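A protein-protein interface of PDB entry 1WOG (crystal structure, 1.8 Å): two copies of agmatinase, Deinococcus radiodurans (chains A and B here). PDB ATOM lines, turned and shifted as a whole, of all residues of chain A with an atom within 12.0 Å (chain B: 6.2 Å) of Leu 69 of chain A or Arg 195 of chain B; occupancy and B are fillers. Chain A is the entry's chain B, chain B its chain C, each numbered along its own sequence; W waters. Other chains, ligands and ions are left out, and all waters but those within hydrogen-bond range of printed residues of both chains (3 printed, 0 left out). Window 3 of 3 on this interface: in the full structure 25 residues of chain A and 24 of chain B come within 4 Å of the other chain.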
ATOM      1  N   PRO A  65      18.908  15.171  33.074  1.00  0.00           N
ATOM      2  CA  PRO A  65      18.577  14.029  32.215  1.00  0.00           C
ATOM      3  C   PRO A  65      17.779  14.452  30.985  1.00  0.00           C
ATOM      4  O   PRO A  65      17.377  15.610  30.870  1.00  0.00           O
ATOM      5  CB  PRO A  65      17.775  13.130  33.148  1.00  0.00           C
ATOM      6  CG  PRO A  65      17.021  14.123  33.960  1.00  0.00           C
ATOM      7  CD  PRO A  65      18.085  15.150  34.297  1.00  0.00           C
ATOM      8  N   PHE A  66      17.538  13.512  30.076  1.00  0.00           N
ATOM      9  CA  PHE A  66      16.809  13.815  28.849  1.00  0.00           C
ATOM     10  C   PHE A  66      15.551  12.987  28.621  1.00  0.00           C
ATOM     11  O   PHE A  66      15.573  11.762  28.725  1.00  0.00           O
ATOM     12  CB  PHE A  66      17.715  13.625  27.625  1.00  0.00           C
ATOM     13  CG  PHE A  66      19.042  14.318  27.728  1.00  0.00           C
ATOM     14  CD1 PHE A  66      20.140  13.667  28.281  1.00  0.00           C
ATOM     15  CD2 PHE A  66      19.196  15.621  27.268  1.00  0.00           C
ATOM     16  CE1 PHE A  66      21.374  14.303  28.375  1.00  0.00           C
ATOM     17  CE2 PHE A  66      20.429  16.268  27.358  1.00  0.00           C
ATOM     18  CZ  PHE A  66      21.517  15.609  27.912  1.00  0.00           C
ATOM     19  N   THR A  67      14.459  13.666  28.296  1.00  0.00           N
ATOM     20  CA  THR A  67      13.202  12.994  27.995  1.00  0.00           C
ATOM     21  C   THR A  67      12.982  13.170  26.499  1.00  0.00           C
ATOM     22  O   THR A  67      12.701  14.276  26.030  1.00  0.00           O
ATOM     23  CB  THR A  67      12.022  13.617  28.760  1.00  0.00           C
ATOM     24  OG1 THR A  67      12.246  13.480  30.167  1.00  0.00           O
ATOM     25  CG2 THR A  67      10.720  12.921  28.388  1.00  0.00           C
ATOM     26  N   GLY A  68      13.126  12.077  25.754  1.00  0.00           N
ATOM     27  CA  GLY A  68      12.966  12.123  24.312  1.00  0.00           C
ATOM     28  C   GLY A  68      11.540  12.273  23.824  1.00  0.00           C
ATOM     29  O   GLY A  68      10.604  12.383  24.616  1.00  0.00           O
ATOM     30  N   LEU A  69      11.382  12.276  22.504  1.00  0.00           N
ATOM     31  CA  LEU A  69      10.076  12.410  21.874  1.00  0.00           C
ATOM     32  C   LEU A  69       9.125  11.295  22.304  1.00  0.00           C
ATOM     33  O   LEU A  69       7.916  11.509  22.414  1.00  0.00           O
ATOM     34  CB  LEU A  69      10.230  12.400  20.350  1.00  0.00           C
ATOM     35  CG  LEU A  69       8.978  12.686  19.518  1.00  0.00           C
ATOM     36  CD1 LEU A  69       8.428  14.058  19.870  1.00  0.00           C
ATOM     37  CD2 LEU A  69       9.323  12.619  18.044  1.00  0.00           C
ATOM     38  N   ASP A  70       9.675  10.109  22.548  1.00  0.00           N
ATOM     39  CA  ASP A  70       8.876   8.961  22.967  1.00  0.00           C
ATOM     40  C   ASP A  70       8.431   9.048  24.426  1.00  0.00           C
ATOM     41  O   ASP A  70       7.695   8.187  24.908  1.00  0.00           O
ATOM     42  CB  ASP A  70       9.659   7.666  22.755  1.00  0.00           C
ATOM     43  CG  ASP A  70      11.028   7.704  23.399  1.00  0.00           C
ATOM     44  OD1 ASP A  70      11.116   8.058  24.592  1.00  0.00           O
ATOM     45  OD2 ASP A  70      12.017   7.373  22.713  1.00  0.00           O
ATOM     46  N   GLY A  71       8.885  10.080  25.130  1.00  0.00           N
ATOM     47  CA  GLY A  71       8.499  10.247  26.521  1.00  0.00           C
ATOM     48  C   GLY A  71       9.386   9.529  27.519  1.00  0.00           C
ATOM     49  O   GLY A  71       9.228   9.703  28.727  1.00  0.00           O
ATOM     50  N   LYS A  72      10.317   8.722  27.021  1.00  0.00           N
ATOM     51  CA  LYS A  72      11.236   7.982  27.879  1.00  0.00           C
ATOM     52  C   LYS A  72      12.391   8.880  28.306  1.00  0.00           C
ATOM     53  O   LYS A  72      12.897   9.675  27.515  1.00  0.00           O
ATOM     54  CB  LYS A  72      11.776   6.758  27.136  1.00  0.00           C
ATOM     55  CG  LYS A  72      10.709   5.736  26.769  1.00  0.00           C
ATOM     56  CD  LYS A  72      11.201   4.720  25.735  1.00  0.00           C
ATOM     57  CE  LYS A  72      12.423   3.940  26.207  1.00  0.00           C
ATOM     58  NZ  LYS A  72      13.669   4.763  26.232  1.00  0.00           N
ATOM     59  N   THR A  73      12.809   8.751  29.560  1.00  0.00           N
ATOM     60  CA  THR A  73      13.900   9.561  30.085  1.00  0.00           C
ATOM     61  C   THR A  73      15.173   8.752  30.281  1.00  0.00           C
ATOM     62  O   THR A  73      15.134   7.607  30.736  1.00  0.00           O
ATOM     63  CB  THR A  73      13.515  10.201  31.435  1.00  0.00           C
ATOM     64  OG1 THR A  73      12.374  11.048  31.255  1.00  0.00           O
ATOM     65  CG2 THR A  73      14.670  11.025  31.985  1.00  0.00           C
ATOM     66  N   ARG A  74      16.301   9.356  29.926  1.00  0.00           N
ATOM     67  CA  ARG A  74      17.595   8.708  30.078  1.00  0.00           C
ATOM     68  C   ARG A  74      18.501   9.552  30.968  1.00  0.00           C
ATOM     69  O   ARG A  74      18.364  10.773  31.029  1.00  0.00           O
ATOM     70  CB  ARG A  74      18.240   8.480  28.707  1.00  0.00           C
ATOM     71  CG  ARG A  74      17.513   7.430  27.872  1.00  0.00           C
ATOM     72  CD  ARG A  74      18.234   7.123  26.570  1.00  0.00           C
ATOM     73  NE  ARG A  74      18.279   8.278  25.679  1.00  0.00           N
ATOM     74  CZ  ARG A  74      18.860   8.276  24.484  1.00  0.00           C
ATOM     75  NH1 ARG A  74      19.450   7.176  24.032  1.00  0.00           N
ATOM     76  NH2 ARG A  74      18.850   9.375  23.739  1.00  0.00           N
ATOM     77  N   ARG A 291      27.070  17.411  22.413  1.00  0.00           N
ATOM     78  CA  ARG A 291      25.887  16.563  22.379  1.00  0.00           C
ATOM     79  C   ARG A 291      26.287  15.103  22.184  1.00  0.00           C
ATOM     80  O   ARG A 291      25.685  14.202  22.779  1.00  0.00           O
ATOM     81  CB  ARG A 291      24.934  16.960  21.248  1.00  0.00           C
ATOM     82  CG  ARG A 291      23.766  15.986  21.151  1.00  0.00           C
ATOM     83  CD  ARG A 291      22.886  16.164  19.935  1.00  0.00           C
ATOM     84  NE  ARG A 291      22.274  14.883  19.585  1.00  0.00           N
ATOM     85  CZ  ARG A 291      21.184  14.740  18.839  1.00  0.00           C
ATOM     86  NH1 ARG A 291      20.556  15.804  18.358  1.00  0.00           N
ATOM     87  NH2 ARG A 291      20.737  13.522  18.555  1.00  0.00           N
ATOM     88  N   GLU A 295      24.945  12.099  24.478  1.00  0.00           N
ATOM     89  CA  GLU A 295      24.142  11.019  23.909  1.00  0.00           C
ATOM     90  C   GLU A 295      24.844   9.677  24.121  1.00  0.00           C
ATOM     91  O   GLU A 295      24.192   8.664  24.359  1.00  0.00           O
ATOM     92  CB  GLU A 295      23.878  11.258  22.408  1.00  0.00           C
ATOM     93  CG  GLU A 295      22.992  10.192  21.744  1.00  0.00           C
ATOM     94  CD  GLU A 295      22.530  10.572  20.338  1.00  0.00           C
ATOM     95  OE1 GLU A 295      21.832   9.754  19.695  1.00  0.00           O
ATOM     96  OE2 GLU A 295      22.860  11.684  19.873  1.00  0.00           O
ATOM     97  N   CYS A 298      24.078   8.625  27.474  1.00  0.00           N
ATOM     98  CA  CYS A 298      22.695   8.150  27.549  1.00  0.00           C
ATOM     99  C   CYS A 298      22.668   6.669  27.191  1.00  0.00           C
ATOM    100  O   CYS A 298      22.013   5.865  27.856  1.00  0.00           O
ATOM    101  CB  CYS A 298      21.791   8.902  26.565  1.00  0.00           C
ATOM    102  SG  CYS A 298      21.301  10.575  27.055  1.00  0.00           S
ATOM    103  N   GLU A 299      23.382   6.321  26.126  1.00  0.00           N
ATOM    104  CA  GLU A 299      23.446   4.942  25.661  1.00  0.00           C
ATOM    105  C   GLU A 299      24.151   4.039  26.670  1.00  0.00           C
ATOM    106  O   GLU A 299      23.716   2.914  26.911  1.00  0.00           O
ATOM    107  CB  GLU A 299      24.182   4.864  24.321  1.00  0.00           C
ATOM    108  CG  GLU A 299      23.547   5.657  23.181  1.00  0.00           C
ATOM    109  CD  GLU A 299      22.175   5.144  22.797  1.00  0.00           C
ATOM    110  OE1 GLU A 299      21.878   3.963  23.065  1.00  0.00           O
ATOM    111  OE2 GLU A 299      21.392   5.920  22.209  1.00  0.00           O
ATOM    112  N   ASP A 302      22.124   3.279  29.745  1.00  0.00           N
ATOM    113  CA  ASP A 302      20.833   2.730  29.360  1.00  0.00           C
ATOM    114  C   ASP A 302      20.956   1.218  29.184  1.00  0.00           C
ATOM    115  O   ASP A 302      19.955   0.516  29.034  1.00  0.00           O
ATOM    116  CB  ASP A 302      20.354   3.371  28.057  1.00  0.00           C
ATOM    117  CG  ASP A 302      18.844   3.417  27.955  1.00  0.00           C
ATOM    118  OD1 ASP A 302      18.326   3.825  26.895  1.00  0.00           O
ATOM    119  OD2 ASP A 302      18.174   3.050  28.942  1.00  0.00           O
ATOM    120  N   LEU B 146       9.490  21.126  18.172  1.00  0.00           N
ATOM    121  CA  LEU B 146       8.028  21.153  18.068  1.00  0.00           C
ATOM    122  C   LEU B 146       7.402  22.536  18.289  1.00  0.00           C
ATOM    123  O   LEU B 146       6.433  22.895  17.620  1.00  0.00           O
ATOM    124  CB  LEU B 146       7.418  20.141  19.054  1.00  0.00           C
ATOM    125  CG  LEU B 146       5.915  19.852  18.957  1.00  0.00           C
ATOM    126  CD1 LEU B 146       5.578  19.238  17.601  1.00  0.00           C
ATOM    127  CD2 LEU B 146       5.511  18.901  20.086  1.00  0.00           C
ATOM    128  N   PHE B 148       5.602  23.734  20.824  1.00  0.00           N
ATOM    129  CA  PHE B 148       4.228  23.667  21.311  1.00  0.00           C
ATOM    130  C   PHE B 148       4.219  23.731  22.834  1.00  0.00           C
ATOM    131  O   PHE B 148       3.275  23.278  23.487  1.00  0.00           O
ATOM    132  CB  PHE B 148       3.573  22.371  20.841  1.00  0.00           C
ATOM    133  CG  PHE B 148       2.080  22.448  20.761  1.00  0.00           C
ATOM    134  CD1 PHE B 148       1.467  23.297  19.841  1.00  0.00           C
ATOM    135  CD2 PHE B 148       1.284  21.684  21.611  1.00  0.00           C
ATOM    136  CE1 PHE B 148       0.075  23.387  19.767  1.00  0.00           C
ATOM    137  CE2 PHE B 148      -0.109  21.766  21.547  1.00  0.00           C
ATOM    138  CZ  PHE B 148      -0.714  22.619  20.622  1.00  0.00           C
ATOM    139  N   LEU B 181      11.641  16.858  13.286  1.00  0.00           N
ATOM    140  CA  LEU B 181      11.939  16.798  14.715  1.00  0.00           C
ATOM    141  C   LEU B 181      13.081  15.850  15.052  1.00  0.00           C
ATOM    142  O   LEU B 181      13.151  14.733  14.543  1.00  0.00           O
ATOM    143  CB  LEU B 181      10.697  16.385  15.511  1.00  0.00           C
ATOM    144  CG  LEU B 181       9.475  17.309  15.482  1.00  0.00           C
ATOM    145  CD1 LEU B 181       8.448  16.804  16.477  1.00  0.00           C
ATOM    146  CD2 LEU B 181       9.881  18.729  15.849  1.00  0.00           C
ATOM    147  N   GLY B 183      16.596  15.462  18.270  1.00  0.00           N
ATOM    148  CA  GLY B 183      17.245  16.028  19.438  1.00  0.00           C
ATOM    149  C   GLY B 183      17.105  15.138  20.656  1.00  0.00           C
ATOM    150  O   GLY B 183      16.284  14.217  20.665  1.00  0.00           O
ATOM    151  N   LEU B 184      17.903  15.419  21.683  1.00  0.00           N
ATOM    152  CA  LEU B 184      17.890  14.635  22.913  1.00  0.00           C
ATOM    153  C   LEU B 184      16.752  15.001  23.850  1.00  0.00           C
ATOM    154  O   LEU B 184      16.256  14.153  24.595  1.00  0.00           O
ATOM    155  CB  LEU B 184      19.212  14.807  23.668  1.00  0.00           C
ATOM    156  CG  LEU B 184      20.490  14.287  23.006  1.00  0.00           C
ATOM    157  CD1 LEU B 184      21.682  14.577  23.905  1.00  0.00           C
ATOM    158  CD2 LEU B 184      20.364  12.796  22.742  1.00  0.00           C
ATOM    159  N   ARG B 185      16.333  16.261  23.806  1.00  0.00           N
ATOM    160  CA  ARG B 185      15.285  16.728  24.700  1.00  0.00           C
ATOM    161  C   ARG B 185      14.023  17.259  24.037  1.00  0.00           C
ATOM    162  O   ARG B 185      14.079  18.038  23.085  1.00  0.00           O
ATOM    163  CB  ARG B 185      15.849  17.815  25.614  1.00  0.00           C
ATOM    164  CG  ARG B 185      14.947  18.188  26.781  1.00  0.00           C
ATOM    165  CD  ARG B 185      15.338  19.534  27.369  1.00  0.00           C
ATOM    166  NE  ARG B 185      16.785  19.686  27.502  1.00  0.00           N
ATOM    167  CZ  ARG B 185      17.554  18.951  28.296  1.00  0.00           C
ATOM    168  NH1 ARG B 185      17.021  17.996  29.047  1.00  0.00           N
ATOM    169  NH2 ARG B 185      18.862  19.171  28.337  1.00  0.00           N
ATOM    170  N   PHE B 186      12.884  16.825  24.561  1.00  0.00           N
ATOM    171  CA  PHE B 186      11.580  17.277  24.093  1.00  0.00           C
ATOM    172  C   PHE B 186      10.704  17.522  25.316  1.00  0.00           C
ATOM    173  O   PHE B 186      10.801  16.803  26.309  1.00  0.00           O
ATOM    174  CB  PHE B 186      10.916  16.240  23.184  1.00  0.00           C
ATOM    175  CG  PHE B 186      11.398  16.284  21.764  1.00  0.00           C
ATOM    176  CD1 PHE B 186      12.541  15.589  21.380  1.00  0.00           C
ATOM    177  CD2 PHE B 186      10.727  17.052  20.817  1.00  0.00           C
ATOM    178  CE1 PHE B 186      13.012  15.659  20.067  1.00  0.00           C
ATOM    179  CE2 PHE B 186      11.187  17.131  19.501  1.00  0.00           C
ATOM    180  CZ  PHE B 186      12.334  16.432  19.127  1.00  0.00           C
ATOM    181  N   ALA B 190       4.371  19.322  26.098  1.00  0.00           N
ATOM    182  CA  ALA B 190       4.093  19.871  24.777  1.00  0.00           C
ATOM    183  C   ALA B 190       3.776  18.755  23.786  1.00  0.00           C
ATOM    184  O   ALA B 190       2.842  18.863  22.996  1.00  0.00           O
ATOM    185  CB  ALA B 190       5.293  20.688  24.287  1.00  0.00           C
ATOM    186  N   VAL B 191       4.563  17.685  23.829  1.00  0.00           N
ATOM    187  CA  VAL B 191       4.346  16.552  22.937  1.00  0.00           C
ATOM    188  C   VAL B 191       2.966  15.957  23.199  1.00  0.00           C
ATOM    189  O   VAL B 191       2.190  15.721  22.272  1.00  0.00           O
ATOM    190  CB  VAL B 191       5.414  15.452  23.155  1.00  0.00           C
ATOM    191  CG1 VAL B 191       5.103  14.245  22.287  1.00  0.00           C
ATOM    192  CG2 VAL B 191       6.800  15.997  22.826  1.00  0.00           C
ATOM    193  N   ALA B 192       2.657  15.728  24.469  1.00  0.00           N
ATOM    194  CA  ALA B 192       1.364  15.158  24.833  1.00  0.00           C
ATOM    195  C   ALA B 192       0.222  16.062  24.384  1.00  0.00           C
ATOM    196  O   ALA B 192      -0.789  15.589  23.860  1.00  0.00           O
ATOM    197  CB  ALA B 192       1.296  14.932  26.342  1.00  0.00           C
ATOM    198  N   ALA B 193       0.388  17.366  24.577  1.00  0.00           N
ATOM    199  CA  ALA B 193      -0.643  18.321  24.193  1.00  0.00           C
ATOM    200  C   ALA B 193      -0.878  18.344  22.685  1.00  0.00           C
ATOM    201  O   ALA B 193      -2.018  18.430  22.229  1.00  0.00           O
ATOM    202  CB  ALA B 193      -0.273  19.717  24.688  1.00  0.00           C
ATOM    203  N   ALA B 194       0.202  18.272  21.912  1.00  0.00           N
ATOM    204  CA  ALA B 194       0.092  18.289  20.459  1.00  0.00           C
ATOM    205  C   ALA B 194      -0.601  17.028  19.952  1.00  0.00           C
ATOM    206  O   ALA B 194      -1.481  17.092  19.090  1.00  0.00           O
ATOM    207  CB  ALA B 194       1.474  18.412  19.833  1.00  0.00           C
ATOM    208  N   ARG B 195      -0.199  15.880  20.487  1.00  0.00           N
ATOM    209  CA  ARG B 195      -0.792  14.615  20.070  1.00  0.00           C
ATOM    210  C   ARG B 195      -2.285  14.601  20.374  1.00  0.00           C
ATOM    211  O   ARG B 195      -3.092  14.169  19.549  1.00  0.00           O
ATOM    212  CB  ARG B 195      -0.101  13.440  20.772  1.00  0.00           C
ATOM    213  CG  ARG B 195       1.366  13.240  20.380  1.00  0.00           C
ATOM    214  CD  ARG B 195       1.932  11.970  21.010  1.00  0.00           C
ATOM    215  NE  ARG B 195       3.363  11.786  20.769  1.00  0.00           N
ATOM    216  CZ  ARG B 195       3.917  11.647  19.567  1.00  0.00           C
ATOM    217  NH1 ARG B 195       3.165  11.672  18.473  1.00  0.00           N
ATOM    218  NH2 ARG B 195       5.226  11.473  19.459  1.00  0.00           N
ATOM    219  N   ALA B 196      -2.651  15.090  21.554  1.00  0.00           N
ATOM    220  CA  ALA B 196      -4.050  15.126  21.963  1.00  0.00           C
ATOM    221  C   ALA B 196      -4.913  15.960  21.021  1.00  0.00           C
ATOM    222  O   ALA B 196      -6.099  15.680  20.847  1.00  0.00           O
ATOM    223  CB  ALA B 196      -4.162  15.657  23.391  1.00  0.00           C
ATOM    224  N   ARG B 197      -4.324  16.984  20.410  1.00  0.00           N
ATOM    225  CA  ARG B 197      -5.070  17.841  19.493  1.00  0.00           C
ATOM    226  C   ARG B 197      -5.091  17.259  18.086  1.00  0.00           C
ATOM    227  O   ARG B 197      -5.613  17.870  17.155  1.00  0.00           O
ATOM    228  CB  ARG B 197      -4.465  19.247  19.464  1.00  0.00           C
ATOM    229  CG  ARG B 197      -4.460  19.947  20.815  1.00  0.00           C
ATOM    230  CD  ARG B 197      -3.834  21.328  20.719  1.00  0.00           C
ATOM    231  NE  ARG B 197      -4.657  22.256  19.950  1.00  0.00           N
ATOM    232  CZ  ARG B 197      -5.782  22.803  20.397  1.00  0.00           C
ATOM    233  NH1 ARG B 197      -6.220  22.518  21.616  1.00  0.00           N
ATOM    234  NH2 ARG B 197      -6.470  23.634  19.627  1.00  0.00           N
ATOM    235  N   GLY B 198      -4.516  16.074  17.932  1.00  0.00           N
ATOM    236  CA  GLY B 198      -4.502  15.434  16.630  1.00  0.00           C
ATOM    237  C   GLY B 198      -3.469  15.973  15.660  1.00  0.00           C
ATOM    238  O   GLY B 198      -3.641  15.852  14.448  1.00  0.00           O
ATOM    239  N   HIS B 199      -2.400  16.574  16.178  1.00  0.00           N
ATOM    240  CA  HIS B 199      -1.343  17.101  15.318  1.00  0.00           C
ATOM    241  C   HIS B 199      -0.467  15.950  14.830  1.00  0.00           C
ATOM    242  O   HIS B 199      -0.363  14.918  15.491  1.00  0.00           O
ATOM    243  CB  HIS B 199      -0.481  18.113  16.078  1.00  0.00           C
ATOM    244  CG  HIS B 199      -1.179  19.403  16.375  1.00  0.00           C
ATOM    245  ND1 HIS B 199      -2.448  19.686  15.920  1.00  0.00           N
ATOM    246  CD2 HIS B 199      -0.778  20.492  17.072  1.00  0.00           C
ATOM    247  CE1 HIS B 199      -2.800  20.894  16.323  1.00  0.00           C
ATOM    248  NE2 HIS B 199      -1.804  21.406  17.024  1.00  0.00           N
ATOM    249  N   ILE B 201       3.201  14.548  14.034  1.00  0.00           N
ATOM    250  CA  ILE B 201       4.606  14.756  14.351  1.00  0.00           C
ATOM    251  C   ILE B 201       5.438  13.790  13.513  1.00  0.00           C
ATOM    252  O   ILE B 201       5.290  12.573  13.636  1.00  0.00           O
ATOM    253  CB  ILE B 201       4.882  14.501  15.851  1.00  0.00           C
ATOM    254  CG1 ILE B 201       4.207  15.584  16.695  1.00  0.00           C
ATOM    255  CG2 ILE B 201       6.377  14.452  16.110  1.00  0.00           C
ATOM    256  CD1 ILE B 201       4.348  15.380  18.200  1.00  0.00           C
ATOM    257  N   ILE B 202       6.308  14.332  12.662  1.00  0.00           N
ATOM    258  CA  ILE B 202       7.147  13.504  11.799  1.00  0.00           C
ATOM    259  C   ILE B 202       8.639  13.701  12.096  1.00  0.00           C
ATOM    260  O   ILE B 202       9.251  14.685  11.672  1.00  0.00           O
ATOM    261  CB  ILE B 202       6.854  13.809  10.307  1.00  0.00           C
ATOM    262  CG1 ILE B 202       5.360  13.617  10.030  1.00  0.00           C
ATOM    263  CG2 ILE B 202       7.657  12.879   9.400  1.00  0.00           C
ATOM    264  CD1 ILE B 202       4.947  13.887   8.596  1.00  0.00           C
ATOM    265  N   PRO B 203       9.239  12.766  12.848  1.00  0.00           N
ATOM    266  CA  PRO B 203      10.662  12.852  13.192  1.00  0.00           C
ATOM    267  C   PRO B 203      11.534  12.796  11.944  1.00  0.00           C
ATOM    268  O   PRO B 203      11.149  12.205  10.934  1.00  0.00           O
ATOM    269  CB  PRO B 203      10.879  11.630  14.088  1.00  0.00           C
ATOM    270  CG  PRO B 203       9.527  11.407  14.703  1.00  0.00           C
ATOM    271  CD  PRO B 203       8.598  11.633  13.539  1.00  0.00           C
HETATM  272  O   HOH W   1      16.793  11.564  24.311  1.00  0.00           O
HETATM  273  O   HOH W   2      14.517  16.540  29.237  1.00  0.00           O
HETATM  274  O   HOH W   3      17.958  12.834  17.596  1.00  0.00           O
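O of Pro 65 of chain A is in hydrogen-bond range of NH1 of Arg 185 of chain B (3.0 Å). O of Thr 67 of chain A lies within hydrogen-bond range of N of Phe 186 of chain B, at 2.9 Å.
OG1 of Thr 67 of chain A lies within hydrogen-bond range of OG1 of Thr 73 of chain A, at 2.7 Å. NH1 of Arg 74 of chain A lies within salt-bridge range of OE2 of Glu 299 of chain A (2.9 Å). The backbone carbonyl oxygen (O) of Phe 66 of chain A sits at hydrogen-bond distance from the backbone NH (N) of Arg 74 of chain A (2.8 Å). NH2 of Arg 291 of chain A is in salt-bridge range of OE2 of Glu 295 of chain A.
Among the printed residues, pairs that only touch across the chains: Phe 66 of chain A with Leu 184 of chain B, Phe 66 of chain A with Arg 185 of chain B, Arg 291 of chain A with Gly 183 of chain B, Leu 69 of chain A with Pro 203 of chain B, Leu 69 of chain A with Phe 186 of chain B, Arg 291 of chain A with Leu 184 of chain B, Thr 67 of chain A with Arg 185 of chain B, Glu 295 of chain A with Leu 184 of chain B, Thr 67 of chain A with Leu 184 of chain B, Arg 74 of chain A with Leu 184 of chain B, Gly 68 of chain A with Leu 184 of chain B, Leu 69 of chain A with Val 191 of chain B, Leu 69 of chain A with Arg 195 of chain B and Leu 69 of chain A with Ile 201 of chain B.
Of chain B, only Phe 186 (3.7 Å), Val 191 (3.9 Å), Arg 195 (3.9 Å), Ile 201 (3.97 Å) and Pro 203 (3.6 Å) come within 4 Å of Leu 69 of chain A. Of chain A, only Leu 69 comes within 4 Å of Arg 195 of chain B. No residue of chain A comes within 4 Å of Leu 181 of chain B. Gly 183 of chain B touches one residue of chain A. Of the printed residues of chain A, Phe 186 of chain B touches Thr 67 and Leu 69. Val 191 of chain B touches one residue of chain A. No residue of chain A comes within 4 Å of Ala 192 of chain B. No residue of chain A comes within 4 Å of Ala 194 of chain B. His 199 of chain B touches none of the printed residues of chain A. Of chain A, only Leu 69 comes within 4 Å of Ile 201 of chain B. Printed residues of chain A within 4 Å of Leu 184 of chain B: Phe 66, Thr 67, Gly 68, Arg 74, Arg 291 and Glu 295. Printed residues of chain B within 4 Å of Arg 74 of chain A: Leu 184. Of the printed residues of chain B, Phe 66 of chain A touches Leu 184 and Arg 185. Of the printed residues of chain B, Thr 67 of chain A touches Leu 184, Arg 185 and Phe 186. Printed residues of chain B within 4 Å of Pro 65 of chain A: Arg 185 (3.0 Å). The nearest residue of chain A that does not touch Arg 195 of chain B is Asp 70 of chain A (5.6 Å). The nearest printed residue of chain B that does not touch Pro 65 of chain A is Leu 184 of chain B (6.5 Å).
Of the 15 printed residues of chain A, 8 touch a printed residue of chain B. Printed residues of chain A that touch a printed residue of chain B: Pro 65, Phe 66, Thr 67, Gly 68, Leu 69, Arg 74, Arg 291 and Glu 295. Of the 20 printed residues of chain B, 8 touch a printed residue of chain A. Printed residues of chain B that touch a printed residue of chain A: Gly 183, Leu 184, Arg 185, Phe 186, Val 191, Arg 195, Ile 201 and Pro 203. Among the printed residues, no Asp or Glu carboxylate lies within 4 Å of a Lys or Arg side-chain nitrogen of the other chain.
No position is printed for both chains. Of the 16 pairs that touch across the chains among the printed residues, none has its exchanged pair printed and touching as well.
Water W1 bridges the backbone carbonyl oxygen (O) of Leu 184 of chain B (2.7 Å) and the guanidinium group (NH2) of Arg 74 of chain A (3.1 Å). Water W2 lies within hydrogen-bond range of NH1 of Arg 185 of chain B (2.9 Å), N of Thr 67 of chain A (3.0 Å) and O of Pro 65 of chain A (3.4 Å). Water W3 lies within hydrogen-bond range of the guanidinium group (NH2) of Arg 291 of chain A and the backbone NH (N) of Gly 183 of chain B.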
